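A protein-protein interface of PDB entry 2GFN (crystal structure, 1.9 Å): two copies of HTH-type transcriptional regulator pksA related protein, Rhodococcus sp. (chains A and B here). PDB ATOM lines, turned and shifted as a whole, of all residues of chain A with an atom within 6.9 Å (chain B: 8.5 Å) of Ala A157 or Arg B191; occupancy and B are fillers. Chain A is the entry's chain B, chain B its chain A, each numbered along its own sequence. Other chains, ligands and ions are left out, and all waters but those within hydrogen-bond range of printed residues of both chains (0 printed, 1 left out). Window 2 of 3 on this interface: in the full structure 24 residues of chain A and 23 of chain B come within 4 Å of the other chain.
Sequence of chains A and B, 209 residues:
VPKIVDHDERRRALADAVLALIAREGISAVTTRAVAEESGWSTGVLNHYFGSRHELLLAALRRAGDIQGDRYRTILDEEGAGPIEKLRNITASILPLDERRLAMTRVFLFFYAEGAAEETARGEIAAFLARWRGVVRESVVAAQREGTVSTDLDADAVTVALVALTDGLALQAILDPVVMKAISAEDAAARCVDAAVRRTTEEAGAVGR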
ATOM      1  N   ASP A 152     -17.497 -20.677 -27.510  1.00  0.00           N
ATOM      2  CA  ASP A 152     -18.411 -19.956 -26.604  1.00  0.00           C
ATOM      3  C   ASP A 152     -18.039 -18.485 -26.359  1.00  0.00           C
ATOM      4  O   ASP A 152     -18.647 -17.790 -25.525  1.00  0.00           O
ATOM      5  CB  ASP A 152     -18.613 -20.716 -25.268  1.00  0.00           C
ATOM      6  CG  ASP A 152     -17.388 -20.654 -24.317  1.00  0.00           C
ATOM      7  OD1 ASP A 152     -16.563 -19.713 -24.367  1.00  0.00           O
ATOM      8  OD2 ASP A 152     -17.265 -21.565 -23.467  1.00  0.00           O
ATOM      9  N   LEU A 153     -17.021 -18.017 -27.057  1.00  0.00           N
ATOM     10  CA  LEU A 153     -16.611 -16.619 -26.896  1.00  0.00           C
ATOM     11  C   LEU A 153     -17.189 -15.836 -28.047  1.00  0.00           C
ATOM     12  O   LEU A 153     -17.364 -16.367 -29.140  1.00  0.00           O
ATOM     13  CB  LEU A 153     -15.095 -16.508 -26.879  1.00  0.00           C
ATOM     14  CG  LEU A 153     -14.406 -17.232 -25.729  1.00  0.00           C
ATOM     15  CD1 LEU A 153     -12.936 -17.243 -26.011  1.00  0.00           C
ATOM     16  CD2 LEU A 153     -14.726 -16.536 -24.379  1.00  0.00           C
ATOM     17  N   ASP A 154     -17.542 -14.592 -27.789  1.00  0.00           N
ATOM     18  CA  ASP A 154     -18.120 -13.760 -28.819  1.00  0.00           C
ATOM     19  C   ASP A 154     -16.987 -13.068 -29.567  1.00  0.00           C
ATOM     20  O   ASP A 154     -16.190 -12.352 -28.968  1.00  0.00           O
ATOM     21  CB  ASP A 154     -19.073 -12.744 -28.214  1.00  0.00           C
ATOM     22  CG  ASP A 154     -19.700 -11.886 -29.259  1.00  0.00           C
ATOM     23  OD1 ASP A 154     -20.796 -12.254 -29.734  1.00  0.00           O
ATOM     24  OD2 ASP A 154     -19.075 -10.897 -29.670  1.00  0.00           O
ATOM     25  N   ALA A 155     -16.893 -13.321 -30.864  1.00  0.00           N
ATOM     26  CA  ALA A 155     -15.767 -12.804 -31.637  1.00  0.00           C
ATOM     27  C   ALA A 155     -15.596 -11.291 -31.518  1.00  0.00           C
ATOM     28  O   ALA A 155     -14.448 -10.789 -31.483  1.00  0.00           O
ATOM     29  CB  ALA A 155     -15.905 -13.197 -33.095  1.00  0.00           C
ATOM     30  N   ASP A 156     -16.711 -10.555 -31.504  1.00  0.00           N
ATOM     31  CA  ASP A 156     -16.609  -9.094 -31.395  1.00  0.00           C
ATOM     32  C   ASP A 156     -16.102  -8.679 -30.017  1.00  0.00           C
ATOM     33  O   ASP A 156     -15.364  -7.702 -29.896  1.00  0.00           O
ATOM     34  CB  ASP A 156     -17.945  -8.389 -31.620  1.00  0.00           C
ATOM     35  CG  ASP A 156     -18.409  -8.440 -33.058  1.00  0.00           C
ATOM     36  OD1 ASP A 156     -17.591  -8.303 -33.995  1.00  0.00           O
ATOM     37  OD2 ASP A 156     -19.632  -8.572 -33.227  1.00  0.00           O
ATOM     38  N   ALA A 157     -16.558  -9.364 -28.969  1.00  0.00           N
ATOM     39  CA  ALA A 157     -16.100  -8.986 -27.621  1.00  0.00           C
ATOM     40  C   ALA A 157     -14.586  -9.262 -27.492  1.00  0.00           C
ATOM     41  O   ALA A 157     -13.838  -8.422 -27.003  1.00  0.00           O
ATOM     42  CB  ALA A 157     -16.886  -9.743 -26.544  1.00  0.00           C
ATOM     43  N   VAL A 158     -14.148 -10.429 -27.951  1.00  0.00           N
ATOM     44  CA  VAL A 158     -12.712 -10.820 -27.929  1.00  0.00           C
ATOM     45  C   VAL A 158     -11.928  -9.721 -28.677  1.00  0.00           C
ATOM     46  O   VAL A 158     -10.862  -9.260 -28.220  1.00  0.00           O
ATOM     47  CB  VAL A 158     -12.504 -12.221 -28.602  1.00  0.00           C
ATOM     48  CG1 VAL A 158     -11.011 -12.508 -28.914  1.00  0.00           C
ATOM     49  CG2 VAL A 158     -13.141 -13.374 -27.744  1.00  0.00           C
ATOM     50  N   THR A 159     -12.450  -9.322 -29.838  1.00  0.00           N
ATOM     51  CA  THR A 159     -11.766  -8.309 -30.680  1.00  0.00           C
ATOM     52  C   THR A 159     -11.608  -6.950 -29.998  1.00  0.00           C
ATOM     53  O   THR A 159     -10.506  -6.366 -30.006  1.00  0.00           O
ATOM     54  CB  THR A 159     -12.495  -8.174 -32.043  1.00  0.00           C
ATOM     55  OG1 THR A 159     -12.389  -9.418 -32.714  1.00  0.00           O
ATOM     56  CG2 THR A 159     -11.911  -7.032 -32.897  1.00  0.00           C
ATOM     57  N   VAL A 160     -12.701  -6.441 -29.423  1.00  0.00           N
ATOM     58  CA  VAL A 160     -12.678  -5.200 -28.686  1.00  0.00           C
ATOM     59  C   VAL A 160     -11.616  -5.304 -27.564  1.00  0.00           C
ATOM     60  O   VAL A 160     -10.831  -4.360 -27.356  1.00  0.00           O
ATOM     61  CB  VAL A 160     -14.117  -4.877 -28.101  1.00  0.00           C
ATOM     62  CG1 VAL A 160     -14.076  -3.772 -27.061  1.00  0.00           C
ATOM     63  CG2 VAL A 160     -15.080  -4.458 -29.221  1.00  0.00           C
ATOM     64  N   ALA A 161     -11.608  -6.437 -26.858  1.00  0.00           N
ATOM     65  CA  ALA A 161     -10.754  -6.590 -25.663  1.00  0.00           C
ATOM     66  C   ALA A 161      -9.290  -6.609 -26.096  1.00  0.00           C
ATOM     67  O   ALA A 161      -8.448  -5.942 -25.502  1.00  0.00           O
ATOM     68  CB  ALA A 161     -11.115  -7.858 -24.873  1.00  0.00           C
ATOM     69  N   LEU A 162      -8.978  -7.391 -27.119  1.00  0.00           N
ATOM     70  CA  LEU A 162      -7.590  -7.492 -27.577  1.00  0.00           C
ATOM     71  C   LEU A 162      -7.069  -6.150 -28.097  1.00  0.00           C
ATOM     72  O   LEU A 162      -5.938  -5.740 -27.791  1.00  0.00           O
ATOM     73  CB  LEU A 162      -7.442  -8.580 -28.649  1.00  0.00           C
ATOM     74  CG  LEU A 162      -6.039  -8.679 -29.252  1.00  0.00           C
ATOM     75  CD1 LEU A 162      -4.995  -9.069 -28.171  1.00  0.00           C
ATOM     76  CD2 LEU A 162      -6.019  -9.723 -30.372  1.00  0.00           C
ATOM     77  N   ALA A 196      -6.907 -12.297 -24.164  1.00  0.00           N
ATOM     78  CA  ALA A 196      -8.104 -11.917 -24.892  1.00  0.00           C
ATOM     79  C   ALA A 196      -8.949 -13.110 -25.323  1.00  0.00           C
ATOM     80  O   ALA A 196     -10.185 -13.055 -25.266  1.00  0.00           O
ATOM     81  CB  ALA A 196      -7.721 -11.063 -26.105  1.00  0.00           C
ATOM     82  N   ARG A 198      -9.143 -15.838 -23.851  1.00  0.00           N
ATOM     83  CA  ARG A 198      -9.401 -16.621 -22.617  1.00  0.00           C
ATOM     84  C   ARG A 198      -8.859 -18.055 -22.743  1.00  0.00           C
ATOM     85  O   ARG A 198      -9.492 -19.028 -22.307  1.00  0.00           O
ATOM     86  CB  ARG A 198     -10.902 -16.596 -22.275  1.00  0.00           C
ATOM     87  CG  ARG A 198     -11.592 -15.245 -22.663  1.00  0.00           C
ATOM     88  CD  ARG A 198     -11.796 -14.247 -21.518  1.00  0.00           C
ATOM     89  NE  ARG A 198     -13.174 -14.309 -21.005  1.00  0.00           N
ATOM     90  CZ  ARG A 198     -13.895 -13.273 -20.555  1.00  0.00           C
ATOM     91  NH1 ARG A 198     -15.132 -13.482 -20.119  1.00  0.00           N
ATOM     92  NH2 ARG A 198     -13.405 -12.029 -20.535  1.00  0.00           N
ATOM     93  N   ARG B  88     -13.271  -5.560  -9.710  1.00  0.00           N
ATOM     94  CA  ARG B  88     -14.341  -5.163 -10.647  1.00  0.00           C
ATOM     95  C   ARG B  88     -14.747  -3.719 -10.358  1.00  0.00           C
ATOM     96  O   ARG B  88     -15.017  -2.928 -11.260  1.00  0.00           O
ATOM     97  CB  ARG B  88     -15.572  -6.063 -10.490  1.00  0.00           C
ATOM     98  CG  ARG B  88     -15.399  -7.489 -10.942  1.00  0.00           C
ATOM     99  CD  ARG B  88     -16.715  -8.253 -10.700  1.00  0.00           C
ATOM    100  NE  ARG B  88     -16.596  -9.664 -11.058  1.00  0.00           N
ATOM    101  CZ  ARG B  88     -17.529 -10.578 -10.826  1.00  0.00           C
ATOM    102  NH1 ARG B  88     -18.652 -10.238 -10.210  1.00  0.00           N
ATOM    103  NH2 ARG B  88     -17.330 -11.832 -11.217  1.00  0.00           N
ATOM    104  N   THR B  91     -12.002  -1.356 -11.511  1.00  0.00           N
ATOM    105  CA  THR B  91     -12.023  -1.284 -12.979  1.00  0.00           C
ATOM    106  C   THR B  91     -13.192  -0.398 -13.455  1.00  0.00           C
ATOM    107  O   THR B  91     -12.994   0.535 -14.233  1.00  0.00           O
ATOM    108  CB  THR B  91     -12.128  -2.704 -13.574  1.00  0.00           C
ATOM    109  OG1 THR B  91     -11.048  -3.515 -13.069  1.00  0.00           O
ATOM    110  CG2 THR B  91     -12.065  -2.672 -15.111  1.00  0.00           C
ATOM    111  N   LEU B 162      -4.426  -5.775 -16.580  1.00  0.00           N
ATOM    112  CA  LEU B 162      -5.758  -5.273 -16.273  1.00  0.00           C
ATOM    113  C   LEU B 162      -5.825  -3.737 -16.441  1.00  0.00           C
ATOM    114  O   LEU B 162      -6.772  -3.185 -17.024  1.00  0.00           O
ATOM    115  CB  LEU B 162      -6.205  -5.714 -14.848  1.00  0.00           C
ATOM    116  CG  LEU B 162      -7.587  -5.177 -14.405  1.00  0.00           C
ATOM    117  CD1 LEU B 162      -8.648  -5.643 -15.370  1.00  0.00           C
ATOM    118  CD2 LEU B 162      -7.881  -5.647 -13.002  1.00  0.00           C
ATOM    119  N   LEU B 165      -5.658  -2.785 -20.180  1.00  0.00           N
ATOM    120  CA  LEU B 165      -6.934  -3.072 -20.850  1.00  0.00           C
ATOM    121  C   LEU B 165      -7.968  -2.026 -20.460  1.00  0.00           C
ATOM    122  O   LEU B 165      -8.695  -1.489 -21.319  1.00  0.00           O
ATOM    123  CB  LEU B 165      -7.412  -4.477 -20.451  1.00  0.00           C
ATOM    124  CG  LEU B 165      -8.865  -4.890 -20.785  1.00  0.00           C
ATOM    125  CD1 LEU B 165      -9.194  -4.933 -22.283  1.00  0.00           C
ATOM    126  CD2 LEU B 165      -9.096  -6.275 -20.188  1.00  0.00           C
ATOM    127  N   THR B 166      -8.038  -1.740 -19.168  1.00  0.00           N
ATOM    128  CA  THR B 166      -9.061  -0.824 -18.651  1.00  0.00           C
ATOM    129  C   THR B 166      -8.813   0.566 -19.254  1.00  0.00           C
ATOM    130  O   THR B 166      -9.754   1.253 -19.649  1.00  0.00           O
ATOM    131  CB  THR B 166      -9.020  -0.688 -17.129  1.00  0.00           C
ATOM    132  OG1 THR B 166      -9.096  -1.977 -16.504  1.00  0.00           O
ATOM    133  CG2 THR B 166     -10.238   0.156 -16.637  1.00  0.00           C
ATOM    134  N   LEU B 169      -9.689   0.763 -22.917  1.00  0.00           N
ATOM    135  CA  LEU B 169     -11.128   0.841 -23.076  1.00  0.00           C
ATOM    136  C   LEU B 169     -11.648   2.225 -22.744  1.00  0.00           C
ATOM    137  O   LEU B 169     -12.497   2.799 -23.474  1.00  0.00           O
ATOM    138  CB  LEU B 169     -11.866  -0.199 -22.175  1.00  0.00           C
ATOM    139  CG  LEU B 169     -11.799  -1.658 -22.668  1.00  0.00           C
ATOM    140  CD1 LEU B 169     -12.366  -2.557 -21.632  1.00  0.00           C
ATOM    141  CD2 LEU B 169     -12.554  -1.891 -24.030  1.00  0.00           C
ATOM    142  N   ALA B 182     -19.658  -0.986 -25.860  1.00  0.00           N
ATOM    143  CA  ALA B 182     -19.069  -2.137 -25.223  1.00  0.00           C
ATOM    144  C   ALA B 182     -18.932  -1.991 -23.687  1.00  0.00           C
ATOM    145  O   ALA B 182     -19.337  -2.885 -22.938  1.00  0.00           O
ATOM    146  CB  ALA B 182     -17.709  -2.456 -25.879  1.00  0.00           C
ATOM    147  N   ALA B 185     -22.070  -2.047 -21.094  1.00  0.00           N
ATOM    148  CA  ALA B 185     -22.676  -3.327 -20.738  1.00  0.00           C
ATOM    149  C   ALA B 185     -22.537  -3.550 -19.229  1.00  0.00           C
ATOM    150  O   ALA B 185     -21.494  -3.231 -18.669  1.00  0.00           O
ATOM    151  CB  ALA B 185     -22.015  -4.448 -21.521  1.00  0.00           C
ATOM    152  N   GLU B 186     -23.576  -4.080 -18.571  1.00  0.00           N
ATOM    153  CA  GLU B 186     -23.500  -4.343 -17.116  1.00  0.00           C
ATOM    154  C   GLU B 186     -22.276  -5.174 -16.693  1.00  0.00           C
ATOM    155  O   GLU B 186     -21.706  -4.952 -15.627  1.00  0.00           O
ATOM    156  CB  GLU B 186     -24.799  -4.981 -16.572  1.00  0.00           C
ATOM    157  CG  GLU B 186     -24.796  -5.208 -15.041  1.00  0.00           C
ATOM    158  CD  GLU B 186     -26.161  -5.583 -14.478  1.00  0.00           C
ATOM    159  OE1 GLU B 186     -26.375  -6.784 -14.175  1.00  0.00           O
ATOM    160  OE2 GLU B 186     -27.025  -4.681 -14.327  1.00  0.00           O
ATOM    161  N   ASP B 187     -21.860  -6.126 -17.515  1.00  0.00           N
ATOM    162  CA  ASP B 187     -20.781  -7.017 -17.098  1.00  0.00           C
ATOM    163  C   ASP B 187     -19.378  -6.598 -17.538  1.00  0.00           C
ATOM    164  O   ASP B 187     -18.439  -7.391 -17.414  1.00  0.00           O
ATOM    165  CB  ASP B 187     -21.064  -8.451 -17.557  1.00  0.00           C
ATOM    166  CG  ASP B 187     -21.134  -8.605 -19.093  1.00  0.00           C
ATOM    167  OD1 ASP B 187     -20.933  -7.623 -19.854  1.00  0.00           O
ATOM    168  OD2 ASP B 187     -21.392  -9.749 -19.537  1.00  0.00           O
ATOM    169  N   ALA B 188     -19.238  -5.372 -18.045  1.00  0.00           N
ATOM    170  CA  ALA B 188     -17.982  -4.918 -18.690  1.00  0.00           C
ATOM    171  C   ALA B 188     -16.752  -4.977 -17.767  1.00  0.00           C
ATOM    172  O   ALA B 188     -15.716  -5.538 -18.140  1.00  0.00           O
ATOM    173  CB  ALA B 188     -18.163  -3.520 -19.257  1.00  0.00           C
ATOM    174  N   ALA B 189     -16.882  -4.453 -16.545  1.00  0.00           N
ATOM    175  CA  ALA B 189     -15.791  -4.526 -15.552  1.00  0.00           C
ATOM    176  C   ALA B 189     -15.456  -5.980 -15.198  1.00  0.00           C
ATOM    177  O   ALA B 189     -14.292  -6.361 -15.098  1.00  0.00           O
ATOM    178  CB  ALA B 189     -16.174  -3.712 -14.288  1.00  0.00           C
ATOM    179  N   ALA B 190     -16.494  -6.815 -15.031  1.00  0.00           N
ATOM    180  CA  ALA B 190     -16.301  -8.204 -14.666  1.00  0.00           C
ATOM    181  C   ALA B 190     -15.581  -8.945 -15.780  1.00  0.00           C
ATOM    182  O   ALA B 190     -14.720  -9.768 -15.508  1.00  0.00           O
ATOM    183  CB  ALA B 190     -17.643  -8.871 -14.310  1.00  0.00           C
ATOM    184  N   ARG B 191     -15.896  -8.610 -17.032  1.00  0.00           N
ATOM    185  CA  ARG B 191     -15.212  -9.194 -18.182  1.00  0.00           C
ATOM    186  C   ARG B 191     -13.732  -8.824 -18.248  1.00  0.00           C
ATOM    187  O   ARG B 191     -12.907  -9.659 -18.622  1.00  0.00           O
ATOM    188  CB  ARG B 191     -15.897  -8.796 -19.491  1.00  0.00           C
ATOM    189  CG  ARG B 191     -17.264  -9.488 -19.732  1.00  0.00           C
ATOM    190  CD  ARG B 191     -17.766  -9.202 -21.166  1.00  0.00           C
ATOM    191  NE  ARG B 191     -17.021 -10.005 -22.137  1.00  0.00           N
ATOM    192  CZ  ARG B 191     -17.561 -10.910 -22.948  1.00  0.00           C
ATOM    193  NH1 ARG B 191     -18.877 -11.141 -22.961  1.00  0.00           N
ATOM    194  NH2 ARG B 191     -16.776 -11.587 -23.776  1.00  0.00           N
ATOM    195  N   CYS B 192     -13.412  -7.574 -17.907  1.00  0.00           N
ATOM    196  CA  CYS B 192     -12.025  -7.086 -17.887  1.00  0.00           C
ATOM    197  C   CYS B 192     -11.213  -7.868 -16.865  1.00  0.00           C
ATOM    198  O   CYS B 192     -10.112  -8.379 -17.161  1.00  0.00           O
ATOM    199  CB  CYS B 192     -11.993  -5.602 -17.536  1.00  0.00           C
ATOM    200  SG  CYS B 192     -12.570  -4.572 -18.859  1.00  0.00           S
ATOM    201  N   VAL B 193     -11.763  -7.975 -15.658  1.00  0.00           N
ATOM    202  CA  VAL B 193     -11.102  -8.685 -14.565  1.00  0.00           C
ATOM    203  C   VAL B 193     -10.893 -10.158 -14.945  1.00  0.00           C
ATOM    204  O   VAL B 193      -9.798 -10.688 -14.810  1.00  0.00           O
ATOM    205  CB  VAL B 193     -11.899  -8.566 -13.219  1.00  0.00           C
ATOM    206  CG1 VAL B 193     -11.326  -9.496 -12.138  1.00  0.00           C
ATOM    207  CG2 VAL B 193     -11.916  -7.119 -12.725  1.00  0.00           C
ATOM    208  N   ASP B 194     -11.936 -10.796 -15.450  1.00  0.00           N
ATOM    209  CA  ASP B 194     -11.836 -12.203 -15.851  1.00  0.00           C
ATOM    210  C   ASP B 194     -10.748 -12.399 -16.907  1.00  0.00           C
ATOM    211  O   ASP B 194      -9.996 -13.391 -16.861  1.00  0.00           O
ATOM    212  CB  ASP B 194     -13.167 -12.715 -16.387  1.00  0.00           C
ATOM    213  CG  ASP B 194     -14.181 -12.993 -15.291  1.00  0.00           C
ATOM    214  OD1 ASP B 194     -13.814 -13.078 -14.091  1.00  0.00           O
ATOM    215  OD2 ASP B 194     -15.363 -13.150 -15.650  1.00  0.00           O
ATOM    216  N   ALA B 195     -10.656 -11.485 -17.867  1.00  0.00           N
ATOM    217  CA  ALA B 195      -9.624 -11.630 -18.890  1.00  0.00           C
ATOM    218  C   ALA B 195      -8.217 -11.566 -18.276  1.00  0.00           C
ATOM    219  O   ALA B 195      -7.310 -12.312 -18.688  1.00  0.00           O
ATOM    220  CB  ALA B 195      -9.797 -10.612 -20.008  1.00  0.00           C
ATOM    221  N   ALA B 196      -8.042 -10.680 -17.291  1.00  0.00           N
ATOM    222  CA  ALA B 196      -6.728 -10.440 -16.675  1.00  0.00           C
ATOM    223  C   ALA B 196      -6.254 -11.572 -15.775  1.00  0.00           C
ATOM    224  O   ALA B 196      -5.099 -11.956 -15.833  1.00  0.00           O
ATOM    225  CB  ALA B 196      -6.716  -9.118 -15.906  1.00  0.00           C
ATOM    226  N   VAL B 197      -7.153 -12.090 -14.941  1.00  0.00           N
ATOM    227  CA  VAL B 197      -6.817 -13.125 -13.965  1.00  0.00           C
ATOM    228  C   VAL B 197      -7.094 -14.525 -14.507  1.00  0.00           C
ATOM    229  O   VAL B 197      -6.859 -15.519 -13.821  1.00  0.00           O
ATOM    230  CB  VAL B 197      -7.602 -12.936 -12.638  1.00  0.00           C
ATOM    231  CG1 VAL B 197      -7.613 -11.457 -12.202  1.00  0.00           C
ATOM    232  CG2 VAL B 197      -9.006 -13.466 -12.779  1.00  0.00           C
ATOM    233  N   ARG B 198      -7.587 -14.592 -15.746  1.00  0.00           N
ATOM    234  CA  ARG B 198      -7.990 -15.850 -16.408  1.00  0.00           C
ATOM    235  C   ARG B 198      -9.137 -16.551 -15.640  1.00  0.00           C
ATOM    236  O   ARG B 198      -8.959 -17.638 -15.068  1.00  0.00           O
ATOM    237  CB  ARG B 198      -6.800 -16.799 -16.675  1.00  0.00           C
ATOM    238  CG  ARG B 198      -5.432 -16.140 -16.962  1.00  0.00           C
ATOM    239  CD  ARG B 198      -5.445 -15.148 -18.138  1.00  0.00           C
ATOM    240  NE  ARG B 198      -4.100 -14.947 -18.692  1.00  0.00           N
ATOM    241  CZ  ARG B 198      -3.401 -13.810 -18.618  1.00  0.00           C
ATOM    242  NH1 ARG B 198      -2.189 -13.760 -19.155  1.00  0.00           N
ATOM    243  NH2 ARG B 198      -3.895 -12.726 -18.022  1.00  0.00           N
ATOM    244  N   ARG B 199     -10.306 -15.904 -15.651  1.00  0.00           N
ATOM    245  CA  ARG B 199     -11.525 -16.328 -14.928  1.00  0.00           C
ATOM    246  C   ARG B 199     -11.268 -16.842 -13.502  1.00  0.00           C
ATOM    247  O   ARG B 199     -11.625 -16.192 -12.510  1.00  0.00           O
ATOM    248  CB  ARG B 199     -12.317 -17.348 -15.758  1.00  0.00           C
ATOM    249  CG  ARG B 199     -13.693 -17.701 -15.216  1.00  0.00           C
ATOM    250  CD  ARG B 199     -14.656 -18.050 -16.354  1.00  0.00           C
ATOM    251  NE  ARG B 199     -15.515 -19.195 -16.045  1.00  0.00           N
ATOM    252  CZ  ARG B 199     -16.560 -19.175 -15.215  1.00  0.00           C
ATOM    253  NH1 ARG B 199     -16.894 -18.056 -14.574  1.00  0.00           N
ATOM    254  NH2 ARG B 199     -17.274 -20.286 -15.013  1.00  0.00           N
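Printed residues of chain B that touch a printed residue of chain A: Leu B165, Leu B169, Arg B191 and Ala B195. Hydrophobic or aromatic side chains of chain B that line the printed part of chain A: Leu B165, Leu B169 and Ala B195. Printed residues of chain A that touch a printed residue of chain B: Ala A157, Val A160, Ala A161 and Arg A198. Hydrophobic or aromatic side chains of chain A within 4 Å of the printed part of chain B: Ala A157 and Val A160. Among the printed residues, 5 pairs touch across the chains. Among the printed residues, no Asp or Glu carboxylate lies within 4 Å of a Lys or Arg side-chain nitrogen of the other chain.
The backbone carbonyl oxygen (O) of Arg B191 is in hydrogen-bond range of the guanidinium group (NH2) of Arg A198 (3.1 Å).
The backbone NH (N) of Ala A157 lies within hydrogen-bond range of the side-chain carboxylate (OD2) of Asp A154 (3.0 Å).
3 positions are printed for both chains.
CB of Ala A157 touches NH2 of Arg B191 (3.3 Å). CD2 of Leu B169 touches CG1 of Val A160 (3.9 Å). Leu B165 touches Ala A161 (CD1 to O, 3.5 Å). Arg A198 touches Ala B195.
Ala A157 touches one residue of chain B. Val A158 touches none of the printed residues of chain B. Printed residues of chain B within 4 Å of Arg A198: Arg B191 and Ala B195. Of the printed residues of chain A, Leu B165 touches Ala A161 (3.5 Å). Of the printed residues of chain A, Leu B169 touches Val A160. Ala B190 touches none of the printed residues of chain A. Of chain A, only Ala A157 (3.3 Å) and Arg A198 (3.1 Å) come within 4 Å of Arg B191. Of the printed residues of chain A, Ala B195 touches Arg A198 (3.9 Å). The nearest residue of chain B that does not touch Ala A157 is Ala B182 (6.9 Å).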
